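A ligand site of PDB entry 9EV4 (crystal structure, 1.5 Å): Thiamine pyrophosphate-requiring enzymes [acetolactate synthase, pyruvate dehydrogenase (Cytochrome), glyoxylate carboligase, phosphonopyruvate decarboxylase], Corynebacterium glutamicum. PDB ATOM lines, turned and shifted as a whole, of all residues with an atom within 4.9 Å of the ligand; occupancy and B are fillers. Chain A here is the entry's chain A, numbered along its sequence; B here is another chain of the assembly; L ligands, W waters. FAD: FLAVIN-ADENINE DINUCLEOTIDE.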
ATOM      1  N   GLY A 211     -23.955  11.061 -22.136  1.00  0.00           N
ATOM      2  CA  GLY A 211     -24.029  10.404 -20.845  1.00  0.00           C
ATOM      3  C   GLY A 211     -22.893  10.840 -19.937  1.00  0.00           C
ATOM      4  O   GLY A 211     -22.192  11.827 -20.227  1.00  0.00           O
ATOM      5  N   ALA A 212     -22.618  10.067 -18.894  1.00  0.00           N
ATOM      6  CA  ALA A 212     -21.588  10.376 -17.904  1.00  0.00           C
ATOM      7  C   ALA A 212     -20.181  10.527 -18.502  1.00  0.00           C
ATOM      8  O   ALA A 212     -19.350  11.202 -17.881  1.00  0.00           O
ATOM      9  CB  ALA A 212     -21.559   9.309 -16.813  1.00  0.00           C
ATOM     10  N   GLY A 213     -19.949   9.966 -19.672  1.00  0.00           N
ATOM     11  CA  GLY A 213     -18.658  10.089 -20.349  1.00  0.00           C
ATOM     12  C   GLY A 213     -18.325  11.496 -20.829  1.00  0.00           C
ATOM     13  O   GLY A 213     -17.189  11.731 -21.260  1.00  0.00           O
ATOM     14  N   HIS A 234     -29.690  14.093 -23.033  1.00  0.00           N
ATOM     15  CA  HIS A 234     -28.837  13.323 -22.124  1.00  0.00           C
ATOM     16  C   HIS A 234     -29.500  12.110 -21.547  1.00  0.00           C
ATOM     17  O   HIS A 234     -30.722  12.050 -21.424  1.00  0.00           O
ATOM     18  CB  HIS A 234     -28.374  14.183 -20.909  1.00  0.00           C
ATOM     19  CG  HIS A 234     -29.494  14.927 -20.226  1.00  0.00           C
ATOM     20  ND1 HIS A 234     -29.819  16.224 -20.584  1.00  0.00           N
ATOM     21  CD2 HIS A 234     -30.305  14.553 -19.208  1.00  0.00           C
ATOM     22  CE1 HIS A 234     -30.805  16.600 -19.785  1.00  0.00           C
ATOM     23  NE2 HIS A 234     -31.140  15.631 -18.927  1.00  0.00           N
ATOM     24  N   ALA A 235     -28.662  11.125 -21.204  1.00  0.00           N
ATOM     25  CA  ALA A 235     -29.080  10.028 -20.354  1.00  0.00           C
ATOM     26  C   ALA A 235     -29.021  10.550 -18.907  1.00  0.00           C
ATOM     27  O   ALA A 235     -28.382  11.574 -18.635  1.00  0.00           O
ATOM     28  CB  ALA A 235     -28.141   8.819 -20.542  1.00  0.00           C
ATOM     29  N   LEU A 236     -29.621   9.846 -17.951  1.00  0.00           N
ATOM     30  CA  LEU A 236     -29.629  10.261 -16.550  1.00  0.00           C
ATOM     31  C   LEU A 236     -28.196  10.441 -16.005  1.00  0.00           C
ATOM     32  O   LEU A 236     -27.958  11.379 -15.228  1.00  0.00           O
ATOM     33  CB  LEU A 236     -30.419   9.254 -15.713  1.00  0.00           C
ATOM     34  CG  LEU A 236     -30.547   9.512 -14.228  1.00  0.00           C
ATOM     35  CD1 LEU A 236     -31.206  10.900 -13.956  1.00  0.00           C
ATOM     36  CD2 LEU A 236     -31.419   8.400 -13.579  1.00  0.00           C
ATOM     37  N   GLY A 237     -27.247   9.575 -16.410  1.00  0.00           N
ATOM     38  CA  GLY A 237     -25.872   9.716 -15.938  1.00  0.00           C
ATOM     39  C   GLY A 237     -25.162  10.960 -16.444  1.00  0.00           C
ATOM     40  O   GLY A 237     -24.132  11.345 -15.887  1.00  0.00           O
ATOM     41  N   GLY A 238     -25.664  11.566 -17.509  1.00  0.00           N
ATOM     42  CA  GLY A 238     -25.047  12.764 -18.060  1.00  0.00           C
ATOM     43  C   GLY A 238     -25.755  14.060 -17.663  1.00  0.00           C
ATOM     44  O   GLY A 238     -25.176  15.133 -17.813  1.00  0.00           O
ATOM     45  N   MET A 252     -34.147  14.642 -21.523  1.00  0.00           N
ATOM     46  CA  MET A 252     -33.750  13.250 -21.272  1.00  0.00           C
ATOM     47  C   MET A 252     -34.721  12.225 -21.881  1.00  0.00           C
ATOM     48  O   MET A 252     -35.933  12.490 -21.942  1.00  0.00           O
ATOM     49  CB  MET A 252     -33.697  13.059 -19.732  1.00  0.00           C
ATOM     50  CG  MET A 252     -33.164  11.701 -19.266  1.00  0.00           C
ATOM     51  SD  MET A 252     -33.032  11.604 -17.453  1.00  0.00           S
ATOM     52  CE  MET A 252     -34.546  10.964 -17.083  1.00  0.00           C
ATOM     53  N   SER A 253     -34.209  11.045 -22.320  1.00  0.00           N
ATOM     54  CA  SER A 253     -35.028   9.943 -22.833  1.00  0.00           C
ATOM     55  C   SER A 253     -35.316   8.916 -21.712  1.00  0.00           C
ATOM     56  O   SER A 253     -34.792   9.041 -20.584  1.00  0.00           O
ATOM     57  CB  SER A 253     -34.334   9.269 -24.024  1.00  0.00           C
ATOM     58  OG  SER A 253     -34.409  10.122 -25.157  1.00  0.00           O
ATOM     59  N   GLY A 254     -36.156   7.914 -22.020  1.00  0.00           N
ATOM     60  CA  GLY A 254     -36.520   6.880 -21.060  1.00  0.00           C
ATOM     61  C   GLY A 254     -37.828   7.203 -20.355  1.00  0.00           C
ATOM     62  O   GLY A 254     -38.378   8.302 -20.547  1.00  0.00           O
ATOM     63  N   LEU A 255     -38.364   6.273 -19.548  1.00  0.00           N
ATOM     64  CA  LEU A 255     -39.658   6.495 -18.878  1.00  0.00           C
ATOM     65  C   LEU A 255     -39.638   7.696 -17.903  1.00  0.00           C
ATOM     66  O   LEU A 255     -40.668   8.343 -17.688  1.00  0.00           O
ATOM     67  CB  LEU A 255     -40.122   5.235 -18.134  1.00  0.00           C
ATOM     68  CG  LEU A 255     -40.617   4.085 -19.057  1.00  0.00           C
ATOM     69  CD1 LEU A 255     -40.929   2.814 -18.231  1.00  0.00           C
ATOM     70  CD2 LEU A 255     -41.898   4.502 -19.801  1.00  0.00           C
ATOM     71  N   LEU A 256     -38.472   8.005 -17.325  1.00  0.00           N
ATOM     72  CA  LEU A 256     -38.372   9.180 -16.419  1.00  0.00           C
ATOM     73  C   LEU A 256     -38.039  10.493 -17.174  1.00  0.00           C
ATOM     74  O   LEU A 256     -37.880  11.550 -16.537  1.00  0.00           O
ATOM     75  CB  LEU A 256     -37.267   8.930 -15.370  1.00  0.00           C
ATOM     76  CG  LEU A 256     -37.670   8.237 -14.083  1.00  0.00           C
ATOM     77  CD1 LEU A 256     -38.500   6.970 -14.326  1.00  0.00           C
ATOM     78  CD2 LEU A 256     -36.436   7.916 -13.229  1.00  0.00           C
ATOM     79  N   GLY A 257     -38.009  10.407 -18.502  1.00  0.00           N
ATOM     80  CA  GLY A 257     -37.646  11.471 -19.410  1.00  0.00           C
ATOM     81  C   GLY A 257     -38.557  12.678 -19.466  1.00  0.00           C
ATOM     82  O   GLY A 257     -39.625  12.733 -18.842  1.00  0.00           O
ATOM     83  N   GLY A 275     -20.336   9.186 -24.942  1.00  0.00           N
ATOM     84  CA  GLY A 275     -20.077   8.755 -23.569  1.00  0.00           C
ATOM     85  C   GLY A 275     -21.336   8.300 -22.841  1.00  0.00           C
ATOM     86  O   GLY A 275     -21.610   8.771 -21.731  1.00  0.00           O
ATOM     87  N   THR A 276     -22.104   7.425 -23.478  1.00  0.00           N
ATOM     88  CA  THR A 276     -23.345   6.928 -22.854  1.00  0.00           C
ATOM     89  C   THR A 276     -23.540   5.452 -23.146  1.00  0.00           C
ATOM     90  O   THR A 276     -23.099   4.952 -24.192  1.00  0.00           O
ATOM     91  CB  THR A 276     -24.570   7.725 -23.341  1.00  0.00           C
ATOM     92  OG1 THR A 276     -25.738   7.232 -22.648  1.00  0.00           O
ATOM     93  CG2 THR A 276     -24.795   7.634 -24.863  1.00  0.00           C
ATOM     94  N   ASP A 277     -24.145   4.753 -22.183  1.00  0.00           N
ATOM     95  CA  ASP A 277     -24.540   3.347 -22.318  1.00  0.00           C
ATOM     96  C   ASP A 277     -26.032   3.201 -21.934  1.00  0.00           C
ATOM     97  O   ASP A 277     -26.465   2.148 -21.436  1.00  0.00           O
ATOM     98  CB  ASP A 277     -23.623   2.448 -21.475  1.00  0.00           C
ATOM     99  CG  ASP A 277     -23.767   0.965 -21.783  1.00  0.00           C
ATOM    100  OD1 ASP A 277     -24.128   0.622 -22.942  1.00  0.00           O
ATOM    101  OD2 ASP A 277     -23.581   0.155 -20.854  1.00  0.00           O
ATOM    102  N   PHE A 278     -26.854   4.271 -22.202  1.00  0.00           N
ATOM    103  CA  PHE A 278     -28.313   4.336 -21.987  1.00  0.00           C
ATOM    104  C   PHE A 278     -28.984   3.047 -22.447  1.00  0.00           C
ATOM    105  O   PHE A 278     -28.850   2.662 -23.604  1.00  0.00           O
ATOM    106  CB  PHE A 278     -28.839   5.516 -22.802  1.00  0.00           C
ATOM    107  CG  PHE A 278     -30.326   5.676 -22.792  1.00  0.00           C
ATOM    108  CD1 PHE A 278     -30.952   6.433 -21.814  1.00  0.00           C
ATOM    109  CD2 PHE A 278     -31.100   5.165 -23.819  1.00  0.00           C
ATOM    110  CE1 PHE A 278     -32.330   6.660 -21.859  1.00  0.00           C
ATOM    111  CE2 PHE A 278     -32.469   5.378 -23.860  1.00  0.00           C
ATOM    112  CZ  PHE A 278     -33.078   6.137 -22.886  1.00  0.00           C
ATOM    113  N   PRO A 279     -29.632   2.309 -21.544  1.00  0.00           N
ATOM    114  CA  PRO A 279     -30.010   0.910 -21.893  1.00  0.00           C
ATOM    115  C   PRO A 279     -31.389   0.681 -22.523  1.00  0.00           C
ATOM    116  O   PRO A 279     -31.679  -0.445 -22.931  1.00  0.00           O
ATOM    117  CB  PRO A 279     -29.954   0.211 -20.525  1.00  0.00           C
ATOM    118  CG  PRO A 279     -30.324   1.299 -19.543  1.00  0.00           C
ATOM    119  CD  PRO A 279     -29.732   2.559 -20.094  1.00  0.00           C
ATOM    120  N   TYR A 280     -32.241   1.733 -22.608  1.00  0.00           N
ATOM    121  CA  TYR A 280     -33.621   1.598 -23.074  1.00  0.00           C
ATOM    122  C   TYR A 280     -33.681   1.756 -24.590  1.00  0.00           C
ATOM    123  O   TYR A 280     -34.066   2.799 -25.119  1.00  0.00           O
ATOM    124  CB  TYR A 280     -34.542   2.580 -22.332  1.00  0.00           C
ATOM    125  CG  TYR A 280     -34.292   2.512 -20.830  1.00  0.00           C
ATOM    126  CD1 TYR A 280     -34.522   1.335 -20.122  1.00  0.00           C
ATOM    127  CD2 TYR A 280     -33.641   3.552 -20.171  1.00  0.00           C
ATOM    128  CE1 TYR A 280     -34.212   1.247 -18.760  1.00  0.00           C
ATOM    129  CE2 TYR A 280     -33.382   3.488 -18.808  1.00  0.00           C
ATOM    130  CZ  TYR A 280     -33.633   2.317 -18.106  1.00  0.00           C
ATOM    131  OH  TYR A 280     -33.356   2.243 -16.766  1.00  0.00           O
ATOM    132  N   VAL A 292     -19.301   7.361 -29.673  1.00  0.00           N
ATOM    133  CA  VAL A 292     -17.963   7.571 -29.152  1.00  0.00           C
ATOM    134  C   VAL A 292     -17.898   7.057 -27.712  1.00  0.00           C
ATOM    135  O   VAL A 292     -18.674   7.530 -26.855  1.00  0.00           O
ATOM    136  CB  VAL A 292     -17.564   9.074 -29.214  1.00  0.00           C
ATOM    137  CG1 VAL A 292     -16.130   9.273 -28.702  1.00  0.00           C
ATOM    138  CG2 VAL A 292     -17.733   9.634 -30.636  1.00  0.00           C
ATOM    139  N   ASP A 293     -17.011   6.077 -27.430  1.00  0.00           N
ATOM    140  CA  ASP A 293     -16.880   5.556 -26.057  1.00  0.00           C
ATOM    141  C   ASP A 293     -15.412   5.216 -25.789  1.00  0.00           C
ATOM    142  O   ASP A 293     -14.710   4.736 -26.698  1.00  0.00           O
ATOM    143  CB  ASP A 293     -17.755   4.315 -25.856  1.00  0.00           C
ATOM    144  CG  ASP A 293     -18.137   4.097 -24.412  1.00  0.00           C
ATOM    145  OD1 ASP A 293     -17.264   3.609 -23.622  1.00  0.00           O
ATOM    146  OD2 ASP A 293     -19.298   4.428 -24.053  1.00  0.00           O
ATOM    147  N   ILE A 294     -14.933   5.492 -24.586  1.00  0.00           N
ATOM    148  CA  ILE A 294     -13.541   5.221 -24.237  1.00  0.00           C
ATOM    149  C   ILE A 294     -13.294   3.677 -24.073  1.00  0.00           C
ATOM    150  O   ILE A 294     -12.159   3.203 -24.224  1.00  0.00           O
ATOM    151  CB  ILE A 294     -13.135   6.006 -22.982  1.00  0.00           C
ATOM    152  CG1 ILE A 294     -11.592   6.147 -22.898  1.00  0.00           C
ATOM    153  CG2 ILE A 294     -13.757   5.397 -21.724  1.00  0.00           C
ATOM    154  CD1 ILE A 294     -11.137   7.248 -22.007  1.00  0.00           C
ATOM    155  N   ASN A 295     -14.355   2.923 -23.840  1.00  0.00           N
ATOM    156  CA  ASN A 295     -14.254   1.470 -23.764  1.00  0.00           C
ATOM    157  C   ASN A 295     -14.935   0.896 -25.022  1.00  0.00           C
ATOM    158  O   ASN A 295     -16.172   0.908 -25.135  1.00  0.00           O
ATOM    159  CB  ASN A 295     -14.884   0.942 -22.478  1.00  0.00           C
ATOM    160  CG  ASN A 295     -14.708  -0.570 -22.336  1.00  0.00           C
ATOM    161  OD1 ASN A 295     -14.585  -1.299 -23.323  1.00  0.00           O
ATOM    162  ND2 ASN A 295     -14.647  -1.053 -21.084  1.00  0.00           N
ATOM    163  N   HIS A 298     -18.074  -1.369 -25.105  1.00  0.00           N
ATOM    164  CA  HIS A 298     -19.409  -0.808 -24.877  1.00  0.00           C
ATOM    165  C   HIS A 298     -20.099  -0.349 -26.157  1.00  0.00           C
ATOM    166  O   HIS A 298     -21.312  -0.087 -26.136  1.00  0.00           O
ATOM    167  CB  HIS A 298     -19.304   0.409 -23.912  1.00  0.00           C
ATOM    168  CG  HIS A 298     -18.812   0.043 -22.542  1.00  0.00           C
ATOM    169  ND1 HIS A 298     -18.910   0.959 -21.488  1.00  0.00           N
ATOM    170  CD2 HIS A 298     -18.267  -1.107 -22.072  1.00  0.00           C
ATOM    171  CE1 HIS A 298     -18.378   0.351 -20.445  1.00  0.00           C
ATOM    172  NE2 HIS A 298     -17.958  -0.896 -20.752  1.00  0.00           N
ATOM    173  N   GLY A 311     -12.547   6.088 -28.102  1.00  0.00           N
ATOM    174  CA  GLY A 311     -11.732   7.218 -27.697  1.00  0.00           C
ATOM    175  C   GLY A 311     -12.415   8.084 -26.661  1.00  0.00           C
ATOM    176  O   GLY A 311     -13.583   7.901 -26.318  1.00  0.00           O
ATOM    177  N   ASP A 312     -11.649   9.006 -26.116  1.00  0.00           N
ATOM    178  CA  ASP A 312     -12.165   9.965 -25.129  1.00  0.00           C
ATOM    179  C   ASP A 312     -13.090  10.976 -25.847  1.00  0.00           C
ATOM    180  O   ASP A 312     -12.745  11.389 -26.936  1.00  0.00           O
ATOM    181  CB  ASP A 312     -10.958  10.676 -24.532  1.00  0.00           C
ATOM    182  CG  ASP A 312     -11.337  11.847 -23.651  1.00  0.00           C
ATOM    183  OD1 ASP A 312     -11.925  11.615 -22.574  1.00  0.00           O
ATOM    184  OD2 ASP A 312     -11.081  13.004 -24.069  1.00  0.00           O
ATOM    185  N   VAL A 313     -14.207  11.393 -25.236  1.00  0.00           N
ATOM    186  CA  VAL A 313     -15.086  12.367 -25.916  1.00  0.00           C
ATOM    187  C   VAL A 313     -14.361  13.690 -26.247  1.00  0.00           C
ATOM    188  O   VAL A 313     -14.457  14.164 -27.391  1.00  0.00           O
ATOM    189  CB  VAL A 313     -16.389  12.667 -25.137  1.00  0.00           C
ATOM    190  CG1 VAL A 313     -17.185  13.817 -25.789  1.00  0.00           C
ATOM    191  CG2 VAL A 313     -17.247  11.400 -25.055  1.00  0.00           C
ATOM    192  N   THR A 384     -33.214   4.699  -4.705  1.00  0.00           N
ATOM    193  CA  THR A 384     -33.849   4.105  -5.876  1.00  0.00           C
ATOM    194  C   THR A 384     -35.355   3.986  -5.716  1.00  0.00           C
ATOM    195  O   THR A 384     -35.832   3.511  -4.672  1.00  0.00           O
ATOM    196  CB  THR A 384     -33.273   2.725  -6.157  1.00  0.00           C
ATOM    197  OG1 THR A 384     -31.872   2.886  -6.328  1.00  0.00           O
ATOM    198  CG2 THR A 384     -33.919   2.076  -7.412  1.00  0.00           C
ATOM    199  N   GLY A 385     -36.082   4.444  -6.725  1.00  0.00           N
ATOM    200  CA  GLY A 385     -37.545   4.372  -6.732  1.00  0.00           C
ATOM    201  C   GLY A 385     -38.142   5.692  -7.182  1.00  0.00           C
ATOM    202  O   GLY A 385     -37.583   6.324  -8.103  1.00  0.00           O
ATOM    203  N   ASN A 388     -35.912   8.785  -7.824  1.00  0.00           N
ATOM    204  CA  ASN A 388     -35.224   8.952  -9.108  1.00  0.00           C
ATOM    205  C   ASN A 388     -36.012   9.860 -10.048  1.00  0.00           C
ATOM    206  O   ASN A 388     -35.413  10.624 -10.792  1.00  0.00           O
ATOM    207  CB  ASN A 388     -34.967   7.618  -9.807  1.00  0.00           C
ATOM    208  CG  ASN A 388     -33.969   6.763  -9.083  1.00  0.00           C
ATOM    209  OD1 ASN A 388     -34.321   5.700  -8.622  1.00  0.00           O
ATOM    210  ND2 ASN A 388     -32.721   7.192  -8.993  1.00  0.00           N
ATOM    211  N   SER A 407     -27.976   4.906  -7.109  1.00  0.00           N
ATOM    212  CA  SER A 407     -27.760   3.562  -7.642  1.00  0.00           C
ATOM    213  C   SER A 407     -28.388   3.507  -9.057  1.00  0.00           C
ATOM    214  O   SER A 407     -29.295   2.711  -9.341  1.00  0.00           O
ATOM    215  CB  SER A 407     -28.390   2.528  -6.702  1.00  0.00           C
ATOM    216  OG  SER A 407     -27.942   1.225  -7.061  1.00  0.00           O
ATOM    217  N   PHE A 408     -27.865   4.363  -9.962  1.00  0.00           N
ATOM    218  CA  PHE A 408     -28.486   4.553 -11.268  1.00  0.00           C
ATOM    219  C   PHE A 408     -28.348   3.336 -12.185  1.00  0.00           C
ATOM    220  O   PHE A 408     -29.136   3.192 -13.124  1.00  0.00           O
ATOM    221  CB  PHE A 408     -27.896   5.795 -11.961  1.00  0.00           C
ATOM    222  CG  PHE A 408     -28.038   7.057 -11.120  1.00  0.00           C
ATOM    223  CD1 PHE A 408     -29.265   7.425 -10.596  1.00  0.00           C
ATOM    224  CD2 PHE A 408     -26.921   7.832 -10.810  1.00  0.00           C
ATOM    225  CE1 PHE A 408     -29.385   8.583  -9.832  1.00  0.00           C
ATOM    226  CE2 PHE A 408     -27.050   8.989 -10.035  1.00  0.00           C
ATOM    227  CZ  PHE A 408     -28.291   9.361  -9.558  1.00  0.00           C
ATOM    228  N   ARG A 409     -27.352   2.454 -11.925  1.00  0.00           N
ATOM    229  CA  ARG A 409     -27.116   1.348 -12.851  1.00  0.00           C
ATOM    230  C   ARG A 409     -27.448   0.023 -12.226  1.00  0.00           C
ATOM    231  O   ARG A 409     -28.045  -0.836 -12.871  1.00  0.00           O
ATOM    232  CB  ARG A 409     -25.632   1.393 -13.290  1.00  0.00           C
ATOM    233  CG  ARG A 409     -25.266   2.707 -13.973  1.00  0.00           C
ATOM    234  CD  ARG A 409     -23.813   3.136 -13.739  1.00  0.00           C
ATOM    235  NE  ARG A 409     -23.486   4.385 -14.439  1.00  0.00           N
ATOM    236  CZ  ARG A 409     -23.503   5.587 -13.885  1.00  0.00           C
ATOM    237  NH1 ARG A 409     -23.803   5.731 -12.586  1.00  0.00           N
ATOM    238  NH2 ARG A 409     -23.215   6.669 -14.602  1.00  0.00           N
ATOM    239  N   GLY A 411     -29.297  -0.225  -9.495  1.00  0.00           N
ATOM    240  CA  GLY A 411     -30.703  -0.050  -9.152  1.00  0.00           C
ATOM    241  C   GLY A 411     -31.138  -0.712  -7.855  1.00  0.00           C
ATOM    242  O   GLY A 411     -32.249  -1.269  -7.798  1.00  0.00           O
ATOM    243  N   PHE B 113     -29.640  -2.656 -17.004  1.00  0.00           N
ATOM    244  CA  PHE B 113     -30.036  -2.100 -15.691  1.00  0.00           C
ATOM    245  C   PHE B 113     -30.362  -3.255 -14.716  1.00  0.00           C
ATOM    246  O   PHE B 113     -31.077  -4.205 -15.117  1.00  0.00           O
ATOM    247  CB  PHE B 113     -31.310  -1.246 -15.922  1.00  0.00           C
ATOM    248  CG  PHE B 113     -31.925  -0.689 -14.655  1.00  0.00           C
ATOM    249  CD1 PHE B 113     -31.203   0.164 -13.830  1.00  0.00           C
ATOM    250  CD2 PHE B 113     -33.234  -0.993 -14.312  1.00  0.00           C
ATOM    251  CE1 PHE B 113     -31.771   0.673 -12.655  1.00  0.00           C
ATOM    252  CE2 PHE B 113     -33.803  -0.468 -13.152  1.00  0.00           C
ATOM    253  CZ  PHE B 113     -33.066   0.352 -12.331  1.00  0.00           C
HETATM  254  PA  FAD L   1     -23.226   4.930 -18.091  1.00  0.00           P
HETATM  255  O1A FAD L   1     -24.201   3.856 -18.375  1.00  0.00           O
HETATM  256  O2A FAD L   1     -22.277   4.813 -16.957  1.00  0.00           O
HETATM  257  O5B FAD L   1     -22.394   5.140 -19.444  1.00  0.00           O
HETATM  258  C5B FAD L   1     -21.262   6.025 -19.475  1.00  0.00           C
HETATM  259  C4B FAD L   1     -20.472   5.657 -20.702  1.00  0.00           C
HETATM  260  O4B FAD L   1     -19.445   6.655 -20.904  1.00  0.00           O
HETATM  261  C3B FAD L   1     -19.756   4.298 -20.595  1.00  0.00           C
HETATM  262  O3B FAD L   1     -20.005   3.461 -21.726  1.00  0.00           O
HETATM  263  C2B FAD L   1     -18.287   4.679 -20.430  1.00  0.00           C
HETATM  264  O2B FAD L   1     -17.385   3.701 -20.939  1.00  0.00           O
HETATM  265  C1B FAD L   1     -18.236   5.993 -21.217  1.00  0.00           C
HETATM  266  N9A FAD L   1     -17.117   6.872 -20.876  1.00  0.00           N
HETATM  267  C8A FAD L   1     -16.645   7.200 -19.631  1.00  0.00           C
HETATM  268  N7A FAD L   1     -15.732   8.148 -19.641  1.00  0.00           N
HETATM  269  C5A FAD L   1     -15.598   8.452 -20.982  1.00  0.00           C
HETATM  270  C6A FAD L   1     -14.772   9.365 -21.672  1.00  0.00           C
HETATM  271  N6A FAD L   1     -13.870  10.142 -21.075  1.00  0.00           N
HETATM  272  N1A FAD L   1     -14.874   9.413 -23.023  1.00  0.00           N
HETATM  273  C2A FAD L   1     -15.732   8.598 -23.628  1.00  0.00           C
HETATM  274  N3A FAD L   1     -16.565   7.690 -23.090  1.00  0.00           N
HETATM  275  C4A FAD L   1     -16.435   7.668 -21.757  1.00  0.00           C
HETATM  276  N1  FAD L   1     -31.831   6.644 -17.224  1.00  0.00           N
HETATM  277  C2  FAD L   1     -32.381   7.393 -18.208  1.00  0.00           C
HETATM  278  O2  FAD L   1     -31.681   8.072 -18.952  1.00  0.00           O
HETATM  279  N3  FAD L   1     -33.749   7.427 -18.366  1.00  0.00           N
HETATM  280  C4  FAD L   1     -34.672   6.771 -17.565  1.00  0.00           C
HETATM  281  O4  FAD L   1     -35.862   6.855 -17.818  1.00  0.00           O
HETATM  282  C4X FAD L   1     -34.087   5.993 -16.496  1.00  0.00           C
HETATM  283  N5  FAD L   1     -34.888   5.446 -15.623  1.00  0.00           N
HETATM  284  C5X FAD L   1     -34.324   4.870 -14.475  1.00  0.00           C
HETATM  285  C6  FAD L   1     -35.168   4.477 -13.432  1.00  0.00           C
HETATM  286  C7  FAD L   1     -34.655   4.058 -12.202  1.00  0.00           C
HETATM  287  C7M FAD L   1     -35.605   3.703 -11.089  1.00  0.00           C
HETATM  288  C8  FAD L   1     -33.254   4.009 -12.022  1.00  0.00           C
HETATM  289  C8M FAD L   1     -32.649   3.602 -10.698  1.00  0.00           C
HETATM  290  C9  FAD L   1     -32.412   4.367 -13.063  1.00  0.00           C
HETATM  291  C9A FAD L   1     -32.931   4.806 -14.285  1.00  0.00           C
HETATM  292  N10 FAD L   1     -32.098   5.325 -15.312  1.00  0.00           N
HETATM  293  C10 FAD L   1     -32.643   5.974 -16.403  1.00  0.00           C
HETATM  294  C1' FAD L   1     -30.666   5.034 -15.337  1.00  0.00           C
HETATM  295  C2' FAD L   1     -30.297   4.081 -16.476  1.00  0.00           C
HETATM  296  O2' FAD L   1     -30.609   2.739 -16.103  1.00  0.00           O
HETATM  297  C3' FAD L   1     -28.802   4.198 -16.800  1.00  0.00           C
HETATM  298  O3' FAD L   1     -28.011   3.906 -15.644  1.00  0.00           O
HETATM  299  C4' FAD L   1     -28.350   5.560 -17.350  1.00  0.00           C
HETATM  300  O4' FAD L   1     -29.260   6.010 -18.368  1.00  0.00           O
HETATM  301  C5' FAD L   1     -26.948   5.483 -17.896  1.00  0.00           C
HETATM  302  O5' FAD L   1     -26.430   6.824 -17.950  1.00  0.00           O
HETATM  303  P   FAD L   1     -25.096   7.124 -18.759  1.00  0.00           P
HETATM  304  O1P FAD L   1     -24.740   8.563 -18.575  1.00  0.00           O
HETATM  305  O2P FAD L   1     -25.184   6.536 -20.106  1.00  0.00           O
HETATM  306  O3P FAD L   1     -23.991   6.327 -17.910  1.00  0.00           O
HETATM  307  O   HOH W   1     -12.191   8.860 -18.431  1.00  0.00           O
HETATM  308  O   HOH W   2     -18.279   6.890 -16.705  1.00  0.00           O
HETATM  309  O   HOH W   3     -15.291  13.154 -20.091  1.00  0.00           O
HETATM  310  O   HOH W   4     -14.997   9.556 -17.087  1.00  0.00           O
HETATM  311  O   HOH W   5     -28.242   0.878 -16.299  1.00  0.00           O
HETATM  312  O   HOH W   6     -37.086   3.479 -16.662  1.00  0.00           O
HETATM  313  O   HOH W   7     -15.329   3.126 -19.035  1.00  0.00           O
HETATM  314  O   HOH W   8     -13.911  11.720 -18.263  1.00  0.00           O
HETATM  315  O   HOH W   9     -23.104   1.279 -18.333  1.00  0.00           O
HETATM  316  O   HOH W  10     -26.376   2.003 -18.605  1.00  0.00           O
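N of Gly 311 sits at hydrogen-bond distance from O of Asp 293 (2.9 Å).
The side-chain carboxylate of Asp 293 is in hydrogen-bond range of the backbone NH of Asn 295.
The backbone NH (N) of Phe 278 is in hydrogen-bond range of the side-chain hydroxyl (OG1) of Thr 276 (3.2 Å).
The side-chain amide nitrogen of Asn 295 sits at hydrogen-bond distance from a ring nitrogen (NE2) of His 298 (3.3 Å).
O of Gly 311 is in hydrogen-bond range of N of Ile 294.
O of Gly 275 sits at hydrogen-bond distance from N of Gly 213 (2.9 Å).
The backbone NH (N) of Gly 275 sits at hydrogen-bond distance from the backbone carbonyl oxygen (O) of Val 292 (3.0 Å).
The backbone NH (N) of Gly 385 sits at hydrogen-bond distance from the side-chain amide oxygen (OD1) of Asn 388, 2.9 Å away.
OD2 of Asp 293 lies within hydrogen-bond range of O3B of the ligand (2.6 Å).
N of Ala 212 lies within hydrogen-bond range of O1P of the ligand (2.6 Å).
O2P of the ligand lies within hydrogen-bond range of OG1 of Thr 276.
A ring nitrogen (ND1) of His 298 lies within hydrogen-bond range of an oxygen (O3B) of the ligand (2.7 Å).
The guanidinium group of Arg 409 is in salt-bridge range of an oxygen (O2A) of the ligand (2.8 Å).
O3' of the ligand lies within hydrogen-bond range of O of Phe 408 (2.9 Å).
The side-chain carboxylate (OD1) of Asp 312 is in hydrogen-bond range of a nitrogen (N6A) of the ligand (2.9 Å).
O2' of the ligand sits at hydrogen-bond distance from OH of Tyr 280.
The backbone NH (N) of Leu 256 sits at hydrogen-bond distance from an oxygen (O4) of the ligand.
N of Leu 236 lies within hydrogen-bond range of O2 of the ligand, at 2.9 Å.
N of Asp 277 lies within hydrogen-bond range of O2P of the ligand, 2.9 Å away.
N3 of the ligand is in hydrogen-bond range of O of Ser 253 (2.9 Å).
The backbone NH of Val 313 is in hydrogen-bond range of a nitrogen (N1A) of the ligand, 3.0 Å away.
N of Gly 237 sits at hydrogen-bond distance from O5' of the ligand, 3.3 Å away.
An oxygen (O4) of the ligand lies within hydrogen-bond range of the backbone NH (N) of Leu 255 (3.1 Å).
N3A of the ligand sits at hydrogen-bond distance from N of Ile 294 (3.1 Å).
The backbone NH (N) of Gly 238 is in hydrogen-bond range of an oxygen (O1P) of the ligand (3.3 Å).
O of Gly 275 sits close to O4B of the ligand, 3.1 Å away.
Merely in contact with the ligand: Gly 211 (3.0 Å), Gly 213 (3.4 Å), Ala 235 (3.5 Å), Met 252 (3.8 Å), Gly 254 (3.2 Å), Phe 278 (3.3 Å), Pro 279 (3.7 Å), Gly 311 (3.5 Å), Thr 384 (3.8 Å), Asn 388 (3.4 Å), Ser 407 (3.7 Å) and Phe 113 of chain B (3.5 Å).
Hydrophobic or aromatic side chains that line the ligand: Ala 212, Ala 235, Leu 236, Met 252, Leu 256, Phe 278, Pro 279, Tyr 280, Ile 294, His 298, Val 313 and Phe 113 of chain B.
Of the 36 residues printed, 30 come within 4 Å of the ligand.
Water W9 lies within hydrogen-bond range of an oxygen (O1A) of the ligand (2.8 Å) and the side-chain carboxylate (OD2) of Asp 277 (2.8 Å).
Water W10 lies within hydrogen-bond range of the backbone carbonyl oxygen (O) of Asp 277 (2.8 Å) and an oxygen (O1A) of the ligand (2.9 Å).
Water W3 lies within hydrogen-bond range of O of Gly 213 and N6A of the ligand.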
